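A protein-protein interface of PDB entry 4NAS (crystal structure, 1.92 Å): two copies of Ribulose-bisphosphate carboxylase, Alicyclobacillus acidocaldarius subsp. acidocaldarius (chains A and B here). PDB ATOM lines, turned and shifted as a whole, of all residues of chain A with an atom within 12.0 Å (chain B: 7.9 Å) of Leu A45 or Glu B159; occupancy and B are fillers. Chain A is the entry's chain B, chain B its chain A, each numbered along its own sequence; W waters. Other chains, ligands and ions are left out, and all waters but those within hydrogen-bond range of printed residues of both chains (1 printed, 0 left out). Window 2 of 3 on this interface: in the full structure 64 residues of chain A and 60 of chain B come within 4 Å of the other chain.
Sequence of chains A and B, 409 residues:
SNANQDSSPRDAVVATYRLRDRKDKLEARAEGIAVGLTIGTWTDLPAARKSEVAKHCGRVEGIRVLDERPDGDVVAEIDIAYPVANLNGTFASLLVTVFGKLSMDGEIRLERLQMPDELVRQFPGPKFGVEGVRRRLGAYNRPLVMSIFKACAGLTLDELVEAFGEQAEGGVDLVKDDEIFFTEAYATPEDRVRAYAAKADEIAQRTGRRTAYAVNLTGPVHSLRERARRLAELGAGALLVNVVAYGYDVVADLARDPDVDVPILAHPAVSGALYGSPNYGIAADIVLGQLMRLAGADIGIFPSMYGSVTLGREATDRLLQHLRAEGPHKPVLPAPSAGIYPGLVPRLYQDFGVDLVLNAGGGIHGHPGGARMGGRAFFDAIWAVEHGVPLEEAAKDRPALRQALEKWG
Ile A39 touches Ala B151. Ile A39 touches Cys B152. Ala B151 touches Thr A41. CG2 of Thr A43 touches CB of Ala B151, 3.6 Å away. Leu A45 touches Leu B155 (CD1 to CD2, 3.9 Å). OE1 of Glu B159 touches CD2 of Leu A45, 3.3 Å away. NH1 of Arg A49 touches CA of Leu B155, at 3.7 Å. CG2 of Val A53 touches CD2 of Leu B155, 3.8 Å away. CD2 of His A56 touches CA of Gly B154, at 3.6 Å.
Printed residues of chain B within 4 Å of Leu A45: Leu B155 (3.9 Å) and Glu B159 (3.3 Å). No residue of chain B comes within 4 Å of Pro A46. No residue of chain A comes within 4 Å of Thr B156. No residue of chain A comes within 4 Å of Leu B157. No residue of chain A comes within 4 Å of Asp B158. No residue of chain A comes within 4 Å of Leu B160. No residue of chain A comes within 4 Å of Val B161. Glu B162 touches none of the printed residues of chain A. No residue of chain A comes within 4 Å of Ala B163. Of the printed residues of chain B, Val A53 touches Leu B155 (3.8 Å). Printed residues of chain B within 4 Å of Thr A43: Ala B151. Of the printed residues of chain B, Ile A39 touches Ala B151 and Cys B152. Printed residues of chain B within 4 Å of His A56: Gly B154 (3.6 Å) and Tyr B186 (2.6 Å). The nearest printed residue of chain B that does not touch Thr A41 is Cys B152 (6.2 Å).
N of Thr B156 lies within hydrogen-bond range of OE2 of Glu B159 (2.7 Å).
No position is printed for both chains.
Of the 19 printed residues of chain A, 7 touch a printed residue of chain B. Printed residues of chain A that touch a printed residue of chain B: Ile A39, Thr A41, Thr A43, Leu A45, Arg A49, Val A53 and His A56. Hydrophobic or aromatic side chains of chain A that line the printed part of chain B: Leu A45, Val A53 and His A56. Along chain A the printed residues that touch a printed residue of chain B span positions 39 to 56. Of the 19 printed residues of chain B, 6 touch a printed residue of chain A. Among the printed residues, 12 pairs touch across the chains.
Water W1 lies within hydrogen-bond range of the backbone carbonyl oxygen (O) of Ala B153 (2.9 Å), the backbone carbonyl oxygen (O) of Ile A39 (2.9 Å) and the backbone NH (N) of Cys B152 (3.3 Å).
The guanidinium group (NE) of Arg A49 lies within salt-bridge range of the side-chain carboxylate (OE1) of Glu B159, at 2.7 Å. OH of Tyr B186 is in hydrogen-bond range of NE2 of His A56, 2.6 Å away. The backbone carbonyl oxygen (O) of Gly B154 is in hydrogen-bond range of the guanidinium group (NH1) of Arg A49 (2.7 Å).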
ATOM      1  N   ILE A  39      18.334  -6.851  -6.070  1.00  0.00           N
ATOM      2  CA  ILE A  39      19.047  -6.332  -4.909  1.00  0.00           C
ATOM      3  C   ILE A  39      19.688  -7.428  -4.071  1.00  0.00           C
ATOM      4  O   ILE A  39      20.439  -7.141  -3.126  1.00  0.00           O
ATOM      5  CB  ILE A  39      18.128  -5.484  -3.997  1.00  0.00           C
ATOM      6  CG1 ILE A  39      16.923  -6.306  -3.520  1.00  0.00           C
ATOM      7  CG2 ILE A  39      17.672  -4.245  -4.729  1.00  0.00           C
ATOM      8  CD1 ILE A  39      16.288  -5.772  -2.203  1.00  0.00           C
ATOM      9  N   GLY A  40      19.401  -8.681  -4.406  1.00  0.00           N
ATOM     10  CA  GLY A  40      19.947  -9.798  -3.656  1.00  0.00           C
ATOM     11  C   GLY A  40      19.128 -10.068  -2.413  1.00  0.00           C
ATOM     12  O   GLY A  40      18.458 -11.097  -2.308  1.00  0.00           O
ATOM     13  N   THR A  41      19.178  -9.129  -1.475  1.00  0.00           N
ATOM     14  CA  THR A  41      18.350  -9.190  -0.280  1.00  0.00           C
ATOM     15  C   THR A  41      18.242  -7.808   0.352  1.00  0.00           C
ATOM     16  O   THR A  41      19.048  -6.915   0.068  1.00  0.00           O
ATOM     17  CB  THR A  41      18.909 -10.172   0.772  1.00  0.00           C
ATOM     18  OG1 THR A  41      18.159 -10.041   1.986  1.00  0.00           O
ATOM     19  CG2 THR A  41      20.356  -9.862   1.067  1.00  0.00           C
ATOM     20  N   TRP A  42      17.236  -7.627   1.198  1.00  0.00           N
ATOM     21  CA  TRP A  42      17.097  -6.373   1.916  1.00  0.00           C
ATOM     22  C   TRP A  42      18.181  -6.279   2.969  1.00  0.00           C
ATOM     23  O   TRP A  42      18.538  -7.276   3.592  1.00  0.00           O
ATOM     24  CB  TRP A  42      15.696  -6.238   2.512  1.00  0.00           C
ATOM     25  CG  TRP A  42      14.669  -6.032   1.433  1.00  0.00           C
ATOM     26  CD1 TRP A  42      13.804  -6.961   0.930  1.00  0.00           C
ATOM     27  CD2 TRP A  42      14.445  -4.829   0.690  1.00  0.00           C
ATOM     28  NE1 TRP A  42      13.035  -6.402  -0.065  1.00  0.00           N
ATOM     29  CE2 TRP A  42      13.413  -5.096  -0.235  1.00  0.00           C
ATOM     30  CE3 TRP A  42      15.013  -3.548   0.721  1.00  0.00           C
ATOM     31  CZ2 TRP A  42      12.934  -4.127  -1.119  1.00  0.00           C
ATOM     32  CZ3 TRP A  42      14.536  -2.586  -0.156  1.00  0.00           C
ATOM     33  CH2 TRP A  42      13.505  -2.880  -1.064  1.00  0.00           C
ATOM     34  N   THR A  43      18.708  -5.073   3.163  1.00  0.00           N
ATOM     35  CA  THR A  43      19.790  -4.843   4.119  1.00  0.00           C
ATOM     36  C   THR A  43      19.328  -3.923   5.257  1.00  0.00           C
ATOM     37  O   THR A  43      18.462  -3.070   5.052  1.00  0.00           O
ATOM     38  CB  THR A  43      20.985  -4.182   3.421  1.00  0.00           C
ATOM     39  OG1 THR A  43      20.516  -3.069   2.652  1.00  0.00           O
ATOM     40  CG2 THR A  43      21.657  -5.157   2.484  1.00  0.00           C
ATOM     41  N   ASP A  44      19.912  -4.088   6.440  1.00  0.00           N
ATOM     42  CA  ASP A  44      19.552  -3.253   7.602  1.00  0.00           C
ATOM     43  C   ASP A  44      20.076  -1.810   7.482  1.00  0.00           C
ATOM     44  O   ASP A  44      20.968  -1.403   8.231  1.00  0.00           O
ATOM     45  CB  ASP A  44      20.047  -3.899   8.911  1.00  0.00           C
ATOM     46  CG  ASP A  44      19.445  -3.250  10.163  1.00  0.00           C
ATOM     47  OD1 ASP A  44      18.238  -2.925  10.156  1.00  0.00           O
ATOM     48  OD2 ASP A  44      20.178  -3.074  11.163  1.00  0.00           O
ATOM     49  N   LEU A  45      19.508  -1.050   6.545  1.00  0.00           N
ATOM     50  CA  LEU A  45      19.897   0.343   6.299  1.00  0.00           C
ATOM     51  C   LEU A  45      18.914   1.314   6.953  1.00  0.00           C
ATOM     52  O   LEU A  45      17.813   0.918   7.327  1.00  0.00           O
ATOM     53  CB  LEU A  45      19.940   0.613   4.790  1.00  0.00           C
ATOM     54  CG  LEU A  45      21.029  -0.050   3.940  1.00  0.00           C
ATOM     55  CD1 LEU A  45      20.747   0.172   2.460  1.00  0.00           C
ATOM     56  CD2 LEU A  45      22.408   0.473   4.302  1.00  0.00           C
ATOM     57  N   PRO A  46      19.303   2.595   7.092  1.00  0.00           N
ATOM     58  CA  PRO A  46      18.348   3.574   7.624  1.00  0.00           C
ATOM     59  C   PRO A  46      17.211   3.875   6.655  1.00  0.00           C
ATOM     60  O   PRO A  46      17.223   3.421   5.512  1.00  0.00           O
ATOM     61  CB  PRO A  46      19.208   4.827   7.863  1.00  0.00           C
ATOM     62  CG  PRO A  46      20.415   4.641   6.994  1.00  0.00           C
ATOM     63  CD  PRO A  46      20.659   3.161   6.957  1.00  0.00           C
ATOM     64  N   ALA A  47      16.244   4.652   7.124  1.00  0.00           N
ATOM     65  CA  ALA A  47      14.999   4.904   6.406  1.00  0.00           C
ATOM     66  C   ALA A  47      15.192   5.384   4.968  1.00  0.00           C
ATOM     67  O   ALA A  47      14.634   4.809   4.033  1.00  0.00           O
ATOM     68  CB  ALA A  47      14.137   5.899   7.198  1.00  0.00           C
ATOM     69  N   ALA A  48      15.980   6.441   4.803  1.00  0.00           N
ATOM     70  CA  ALA A  48      16.199   7.045   3.496  1.00  0.00           C
ATOM     71  C   ALA A  48      16.798   6.040   2.532  1.00  0.00           C
ATOM     72  O   ALA A  48      16.336   5.891   1.396  1.00  0.00           O
ATOM     73  CB  ALA A  48      17.102   8.259   3.626  1.00  0.00           C
ATOM     74  N   ARG A  49      17.820   5.334   3.004  1.00  0.00           N
ATOM     75  CA  ARG A  49      18.521   4.356   2.181  1.00  0.00           C
ATOM     76  C   ARG A  49      17.609   3.256   1.638  1.00  0.00           C
ATOM     77  O   ARG A  49      17.768   2.843   0.495  1.00  0.00           O
ATOM     78  CB  ARG A  49      19.695   3.740   2.943  1.00  0.00           C
ATOM     79  CG  ARG A  49      20.853   4.692   3.208  1.00  0.00           C
ATOM     80  CD  ARG A  49      21.527   5.188   1.939  1.00  0.00           C
ATOM     81  NE  ARG A  49      22.021   4.094   1.112  1.00  0.00           N
ATOM     82  CZ  ARG A  49      21.667   3.907  -0.153  1.00  0.00           C
ATOM     83  NH1 ARG A  49      22.151   2.878  -0.837  1.00  0.00           N
ATOM     84  NH2 ARG A  49      20.821   4.749  -0.734  1.00  0.00           N
ATOM     85  N   LYS A  50      16.658   2.787   2.439  1.00  0.00           N
ATOM     86  CA  LYS A  50      15.777   1.704   1.988  1.00  0.00           C
ATOM     87  C   LYS A  50      14.949   2.126   0.768  1.00  0.00           C
ATOM     88  O   LYS A  50      14.876   1.403  -0.244  1.00  0.00           O
ATOM     89  CB  LYS A  50      14.858   1.234   3.116  1.00  0.00           C
ATOM     90  N   SER A  51      14.344   3.306   0.874  1.00  0.00           N
ATOM     91  CA  SER A  51      13.546   3.895  -0.197  1.00  0.00           C
ATOM     92  C   SER A  51      14.352   4.058  -1.489  1.00  0.00           C
ATOM     93  O   SER A  51      13.828   3.862  -2.588  1.00  0.00           O
ATOM     94  CB  SER A  51      12.981   5.247   0.261  1.00  0.00           C
ATOM     95  OG  SER A  51      12.219   5.876  -0.757  1.00  0.00           O
ATOM     96  N   GLU A  52      15.630   4.401  -1.348  1.00  0.00           N
ATOM     97  CA  GLU A  52      16.509   4.594  -2.492  1.00  0.00           C
ATOM     98  C   GLU A  52      16.919   3.255  -3.101  1.00  0.00           C
ATOM     99  O   GLU A  52      16.961   3.104  -4.334  1.00  0.00           O
ATOM    100  CB  GLU A  52      17.746   5.384  -2.072  1.00  0.00           C
ATOM    101  N   VAL A  53      17.210   2.290  -2.231  1.00  0.00           N
ATOM    102  CA  VAL A  53      17.580   0.938  -2.654  1.00  0.00           C
ATOM    103  C   VAL A  53      16.394   0.258  -3.336  1.00  0.00           C
ATOM    104  O   VAL A  53      16.559  -0.517  -4.290  1.00  0.00           O
ATOM    105  CB  VAL A  53      18.081   0.077  -1.451  1.00  0.00           C
ATOM    106  CG1 VAL A  53      18.278  -1.378  -1.848  1.00  0.00           C
ATOM    107  CG2 VAL A  53      19.383   0.649  -0.894  1.00  0.00           C
ATOM    108  N   ALA A  54      15.198   0.580  -2.845  1.00  0.00           N
ATOM    109  CA  ALA A  54      13.950   0.013  -3.347  1.00  0.00           C
ATOM    110  C   ALA A  54      13.821   0.151  -4.858  1.00  0.00           C
ATOM    111  O   ALA A  54      13.289  -0.735  -5.524  1.00  0.00           O
ATOM    112  CB  ALA A  54      12.754   0.657  -2.650  1.00  0.00           C
ATOM    113  N   LYS A  55      14.328   1.257  -5.392  1.00  0.00           N
ATOM    114  CA  LYS A  55      14.249   1.523  -6.823  1.00  0.00           C
ATOM    115  C   LYS A  55      15.098   0.555  -7.648  1.00  0.00           C
ATOM    116  O   LYS A  55      14.930   0.472  -8.860  1.00  0.00           O
ATOM    117  CB  LYS A  55      14.631   2.978  -7.132  1.00  0.00           C
ATOM    118  CG  LYS A  55      16.062   3.169  -7.627  1.00  0.00           C
ATOM    119  CD  LYS A  55      16.112   4.078  -8.849  1.00  0.00           C
ATOM    120  CE  LYS A  55      17.241   3.680  -9.798  1.00  0.00           C
ATOM    121  NZ  LYS A  55      17.219   4.481 -11.059  1.00  0.00           N
ATOM    122  N   HIS A  56      16.000  -0.172  -6.990  1.00  0.00           N
ATOM    123  CA  HIS A  56      16.815  -1.183  -7.655  1.00  0.00           C
ATOM    124  C   HIS A  56      16.195  -2.570  -7.520  1.00  0.00           C
ATOM    125  O   HIS A  56      16.710  -3.555  -8.072  1.00  0.00           O
ATOM    126  CB  HIS A  56      18.239  -1.201  -7.083  1.00  0.00           C
ATOM    127  CG  HIS A  56      19.077  -0.034  -7.501  1.00  0.00           C
ATOM    128  ND1 HIS A  56      19.801  -0.021  -8.675  1.00  0.00           N
ATOM    129  CD2 HIS A  56      19.300   1.164  -6.907  1.00  0.00           C
ATOM    130  CE1 HIS A  56      20.440   1.130  -8.783  1.00  0.00           C
ATOM    131  NE2 HIS A  56      20.153   1.869  -7.722  1.00  0.00           N
ATOM    132  N   CYS A  57      15.090  -2.661  -6.782  1.00  0.00           N
ATOM    133  CA  CYS A  57      14.506  -3.974  -6.531  1.00  0.00           C
ATOM    134  C   CYS A  57      13.563  -4.400  -7.653  1.00  0.00           C
ATOM    135  O   CYS A  57      12.872  -3.570  -8.240  1.00  0.00           O
ATOM    136  CB  CYS A  57      13.791  -4.022  -5.174  1.00  0.00           C
ATOM    137  SG  CYS A  57      13.184  -5.676  -4.737  1.00  0.00           S
ATOM    138  N   PHE B 149      28.679 -11.943  -1.361  1.00  0.00           N
ATOM    139  CA  PHE B 149      27.902 -10.763  -1.000  1.00  0.00           C
ATOM    140  C   PHE B 149      26.414 -11.072  -1.090  1.00  0.00           C
ATOM    141  O   PHE B 149      25.935 -11.693  -2.063  1.00  0.00           O
ATOM    142  CB  PHE B 149      28.200  -9.600  -1.940  1.00  0.00           C
ATOM    143  CG  PHE B 149      29.240  -8.642  -1.436  1.00  0.00           C
ATOM    144  CD1 PHE B 149      30.595  -8.897  -1.636  1.00  0.00           C
ATOM    145  CD2 PHE B 149      28.869  -7.478  -0.792  1.00  0.00           C
ATOM    146  CE1 PHE B 149      31.565  -7.994  -1.171  1.00  0.00           C
ATOM    147  CE2 PHE B 149      29.828  -6.568  -0.334  1.00  0.00           C
ATOM    148  CZ  PHE B 149      31.175  -6.833  -0.534  1.00  0.00           C
ATOM    149  N   ALA B 151      24.070  -8.581  -0.879  1.00  0.00           N
ATOM    150  CA  ALA B 151      23.416  -7.469  -1.571  1.00  0.00           C
ATOM    151  C   ALA B 151      24.457  -6.529  -2.144  1.00  0.00           C
ATOM    152  O   ALA B 151      25.421  -6.196  -1.464  1.00  0.00           O
ATOM    153  CB  ALA B 151      22.494  -6.710  -0.628  1.00  0.00           C
ATOM    154  N   CYS B 152      24.251  -6.096  -3.390  1.00  0.00           N
ATOM    155  CA  CYS B 152      25.223  -5.256  -4.087  1.00  0.00           C
ATOM    156  C   CYS B 152      24.606  -4.053  -4.798  1.00  0.00           C
ATOM    157  O   CYS B 152      24.997  -2.906  -4.545  1.00  0.00           O
ATOM    158  CB  CYS B 152      26.009  -6.081  -5.109  1.00  0.00           C
ATOM    159  SG  CYS B 152      26.858  -7.516  -4.410  1.00  0.00           S
ATOM    160  N   ALA B 153      23.669  -4.317  -5.708  1.00  0.00           N
ATOM    161  CA  ALA B 153      23.105  -3.255  -6.537  1.00  0.00           C
ATOM    162  C   ALA B 153      22.425  -2.211  -5.670  1.00  0.00           C
ATOM    163  O   ALA B 153      21.540  -2.540  -4.874  1.00  0.00           O
ATOM    164  CB  ALA B 153      22.117  -3.817  -7.539  1.00  0.00           C
ATOM    165  N   GLY B 154      22.840  -0.955  -5.825  1.00  0.00           N
ATOM    166  CA  GLY B 154      22.207   0.138  -5.107  1.00  0.00           C
ATOM    167  C   GLY B 154      22.838   0.549  -3.781  1.00  0.00           C
ATOM    168  O   GLY B 154      22.509   1.596  -3.231  1.00  0.00           O
ATOM    169  N   LEU B 155      23.747  -0.254  -3.243  1.00  0.00           N
ATOM    170  CA  LEU B 155      24.434   0.179  -2.026  1.00  0.00           C
ATOM    171  C   LEU B 155      25.653   1.027  -2.391  1.00  0.00           C
ATOM    172  O   LEU B 155      26.226   0.900  -3.484  1.00  0.00           O
ATOM    173  CB  LEU B 155      24.845  -0.996  -1.137  1.00  0.00           C
ATOM    174  CG  LEU B 155      23.819  -2.089  -0.825  1.00  0.00           C
ATOM    175  CD1 LEU B 155      24.285  -2.915   0.377  1.00  0.00           C
ATOM    176  CD2 LEU B 155      22.428  -1.519  -0.587  1.00  0.00           C
ATOM    177  N   THR B 156      26.041   1.900  -1.470  1.00  0.00           N
ATOM    178  CA  THR B 156      27.149   2.816  -1.699  1.00  0.00           C
ATOM    179  C   THR B 156      28.455   2.084  -1.452  1.00  0.00           C
ATOM    180  O   THR B 156      28.471   1.006  -0.829  1.00  0.00           O
ATOM    181  CB  THR B 156      27.078   3.993  -0.713  1.00  0.00           C
ATOM    182  OG1 THR B 156      27.200   3.483   0.618  1.00  0.00           O
ATOM    183  CG2 THR B 156      25.749   4.706  -0.841  1.00  0.00           C
ATOM    184  N   LEU B 157      29.549   2.670  -1.927  1.00  0.00           N
ATOM    185  CA  LEU B 157      30.882   2.106  -1.711  1.00  0.00           C
ATOM    186  C   LEU B 157      31.174   1.860  -0.223  1.00  0.00           C
ATOM    187  O   LEU B 157      31.701   0.810   0.166  1.00  0.00           O
ATOM    188  CB  LEU B 157      31.947   3.036  -2.299  1.00  0.00           C
ATOM    189  CG  LEU B 157      33.382   2.540  -2.124  1.00  0.00           C
ATOM    190  CD1 LEU B 157      33.553   1.207  -2.818  1.00  0.00           C
ATOM    191  CD2 LEU B 157      34.386   3.558  -2.657  1.00  0.00           C
ATOM    192  N   ASP B 158      30.825   2.825   0.619  1.00  0.00           N
ATOM    193  CA  ASP B 158      31.072   2.656   2.048  1.00  0.00           C
ATOM    194  C   ASP B 158      30.262   1.492   2.625  1.00  0.00           C
ATOM    195  O   ASP B 158      30.774   0.718   3.431  1.00  0.00           O
ATOM    196  CB  ASP B 158      30.776   3.940   2.822  1.00  0.00           C
ATOM    197  CG  ASP B 158      31.752   5.058   2.500  1.00  0.00           C
ATOM    198  OD1 ASP B 158      32.809   4.783   1.894  1.00  0.00           O
ATOM    199  OD2 ASP B 158      31.455   6.218   2.857  1.00  0.00           O
ATOM    200  N   GLU B 159      29.001   1.378   2.210  1.00  0.00           N
ATOM    201  CA  GLU B 159      28.121   0.309   2.687  1.00  0.00           C
ATOM    202  C   GLU B 159      28.660  -1.040   2.198  1.00  0.00           C
ATOM    203  O   GLU B 159      28.579  -2.067   2.882  1.00  0.00           O
ATOM    204  CB  GLU B 159      26.683   0.545   2.198  1.00  0.00           C
ATOM    205  CG  GLU B 159      25.953   1.691   2.885  1.00  0.00           C
ATOM    206  CD  GLU B 159      24.766   2.230   2.086  1.00  0.00           C
ATOM    207  OE1 GLU B 159      23.910   2.924   2.687  1.00  0.00           O
ATOM    208  OE2 GLU B 159      24.691   1.977   0.860  1.00  0.00           O
ATOM    209  N   LEU B 160      29.245  -1.019   1.010  1.00  0.00           N
ATOM    210  CA  LEU B 160      29.834  -2.216   0.432  1.00  0.00           C
ATOM    211  C   LEU B 160      31.128  -2.622   1.145  1.00  0.00           C
ATOM    212  O   LEU B 160      31.399  -3.821   1.310  1.00  0.00           O
ATOM    213  CB  LEU B 160      30.064  -2.012  -1.067  1.00  0.00           C
ATOM    214  CG  LEU B 160      28.809  -2.032  -1.954  1.00  0.00           C
ATOM    215  CD1 LEU B 160      29.116  -1.428  -3.331  1.00  0.00           C
ATOM    216  CD2 LEU B 160      28.238  -3.441  -2.113  1.00  0.00           C
ATOM    217  N   VAL B 161      31.908  -1.628   1.581  1.00  0.00           N
ATOM    218  CA  VAL B 161      33.148  -1.873   2.320  1.00  0.00           C
ATOM    219  C   VAL B 161      32.857  -2.502   3.683  1.00  0.00           C
ATOM    220  O   VAL B 161      33.520  -3.447   4.104  1.00  0.00           O
ATOM    221  CB  VAL B 161      33.959  -0.570   2.527  1.00  0.00           C
ATOM    222  CG1 VAL B 161      35.098  -0.784   3.539  1.00  0.00           C
ATOM    223  CG2 VAL B 161      34.508  -0.048   1.211  1.00  0.00           C
ATOM    224  N   GLU B 162      31.867  -1.958   4.378  1.00  0.00           N
ATOM    225  CA  GLU B 162      31.412  -2.528   5.642  1.00  0.00           C
ATOM    226  C   GLU B 162      30.938  -3.978   5.464  1.00  0.00           C
ATOM    227  O   GLU B 162      31.272  -4.847   6.262  1.00  0.00           O
ATOM    228  CB  GLU B 162      30.310  -1.651   6.239  1.00  0.00           C
ATOM    229  CG  GLU B 162      29.547  -2.243   7.411  1.00  0.00           C
ATOM    230  CD  GLU B 162      28.898  -1.159   8.279  1.00  0.00           C
ATOM    231  OE1 GLU B 162      28.777  -0.009   7.798  1.00  0.00           O
ATOM    232  OE2 GLU B 162      28.518  -1.449   9.438  1.00  0.00           O
ATOM    233  N   ALA B 163      30.167  -4.231   4.413  1.00  0.00           N
ATOM    234  CA  ALA B 163      29.707  -5.593   4.120  1.00  0.00           C
ATOM    235  C   ALA B 163      30.875  -6.550   3.912  1.00  0.00           C
ATOM    236  O   ALA B 163      30.915  -7.629   4.511  1.00  0.00           O
ATOM    237  CB  ALA B 163      28.790  -5.615   2.909  1.00  0.00           C
ATOM    238  N   PHE B 164      31.821  -6.155   3.063  1.00  0.00           N
ATOM    239  CA  PHE B 164      32.999  -6.980   2.816  1.00  0.00           C
ATOM    240  C   PHE B 164      33.737  -7.242   4.130  1.00  0.00           C
ATOM    241  O   PHE B 164      34.216  -8.347   4.378  1.00  0.00           O
ATOM    242  CB  PHE B 164      33.938  -6.320   1.805  1.00  0.00           C
ATOM    243  CG  PHE B 164      35.291  -6.978   1.716  1.00  0.00           C
ATOM    244  CD1 PHE B 164      36.339  -6.580   2.552  1.00  0.00           C
ATOM    245  CD2 PHE B 164      35.521  -7.983   0.798  1.00  0.00           C
ATOM    246  CE1 PHE B 164      37.590  -7.182   2.480  1.00  0.00           C
ATOM    247  CE2 PHE B 164      36.768  -8.589   0.714  1.00  0.00           C
ATOM    248  CZ  PHE B 164      37.806  -8.196   1.566  1.00  0.00           C
ATOM    249  N   GLY B 165      33.826  -6.211   4.965  1.00  0.00           N
ATOM    250  CA  GLY B 165      34.472  -6.347   6.256  1.00  0.00           C
ATOM    251  C   GLY B 165      33.870  -7.435   7.122  1.00  0.00           C
ATOM    252  O   GLY B 165      34.595  -8.237   7.727  1.00  0.00           O
ATOM    253  N   GLU B 166      32.544  -7.474   7.181  1.00  0.00           N
ATOM    254  CA  GLU B 166      31.841  -8.428   8.040  1.00  0.00           C
ATOM    255  C   GLU B 166      32.160  -9.858   7.662  1.00  0.00           C
ATOM    256  O   GLU B 166      32.403 -10.699   8.523  1.00  0.00           O
ATOM    257  CB  GLU B 166      30.333  -8.215   7.981  1.00  0.00           C
ATOM    258  CG  GLU B 166      29.785  -7.260   9.025  1.00  0.00           C
ATOM    259  CD  GLU B 166      28.288  -7.439   9.218  1.00  0.00           C
ATOM    260  OE1 GLU B 166      27.837  -8.596   9.404  1.00  0.00           O
ATOM    261  OE2 GLU B 166      27.561  -6.423   9.173  1.00  0.00           O
ATOM    262  N   TYR B 186      27.304   3.256  -8.395  1.00  0.00           N
ATOM    263  CA  TYR B 186      27.618   3.589  -6.999  1.00  0.00           C
ATOM    264  C   TYR B 186      29.076   3.309  -6.663  1.00  0.00           C
ATOM    265  O   TYR B 186      29.735   4.110  -6.023  1.00  0.00           O
ATOM    266  CB  TYR B 186      26.710   2.847  -6.016  1.00  0.00           C
ATOM    267  CG  TYR B 186      25.240   3.184  -6.163  1.00  0.00           C
ATOM    268  CD1 TYR B 186      24.472   2.586  -7.158  1.00  0.00           C
ATOM    269  CD2 TYR B 186      24.615   4.084  -5.306  1.00  0.00           C
ATOM    270  CE1 TYR B 186      23.136   2.876  -7.305  1.00  0.00           C
ATOM    271  CE2 TYR B 186      23.264   4.383  -5.449  1.00  0.00           C
ATOM    272  CZ  TYR B 186      22.533   3.771  -6.462  1.00  0.00           C
ATOM    273  OH  TYR B 186      21.188   4.044  -6.646  1.00  0.00           O
ATOM    274  N   TYR B 196      38.307  -2.704  -0.948  1.00  0.00           N
ATOM    275  CA  TYR B 196      38.236  -3.999  -0.264  1.00  0.00           C
ATOM    276  C   TYR B 196      39.631  -4.504   0.094  1.00  0.00           C
ATOM    277  O   TYR B 196      39.829  -5.096   1.155  1.00  0.00           O
ATOM    278  CB  TYR B 196      37.518  -5.073  -1.096  1.00  0.00           C
ATOM    279  CG  TYR B 196      36.067  -4.797  -1.427  1.00  0.00           C
ATOM    280  CD1 TYR B 196      35.428  -3.638  -0.996  1.00  0.00           C
ATOM    281  CD2 TYR B 196      35.327  -5.713  -2.178  1.00  0.00           C
ATOM    282  CE1 TYR B 196      34.099  -3.388  -1.327  1.00  0.00           C
ATOM    283  CE2 TYR B 196      34.003  -5.476  -2.498  1.00  0.00           C
ATOM    284  CZ  TYR B 196      33.391  -4.316  -2.069  1.00  0.00           C
ATOM    285  OH  TYR B 196      32.067  -4.092  -2.398  1.00  0.00           O
HETATM  286  O   HOH W   1      21.435  -4.429  -2.716  1.00  0.00           O
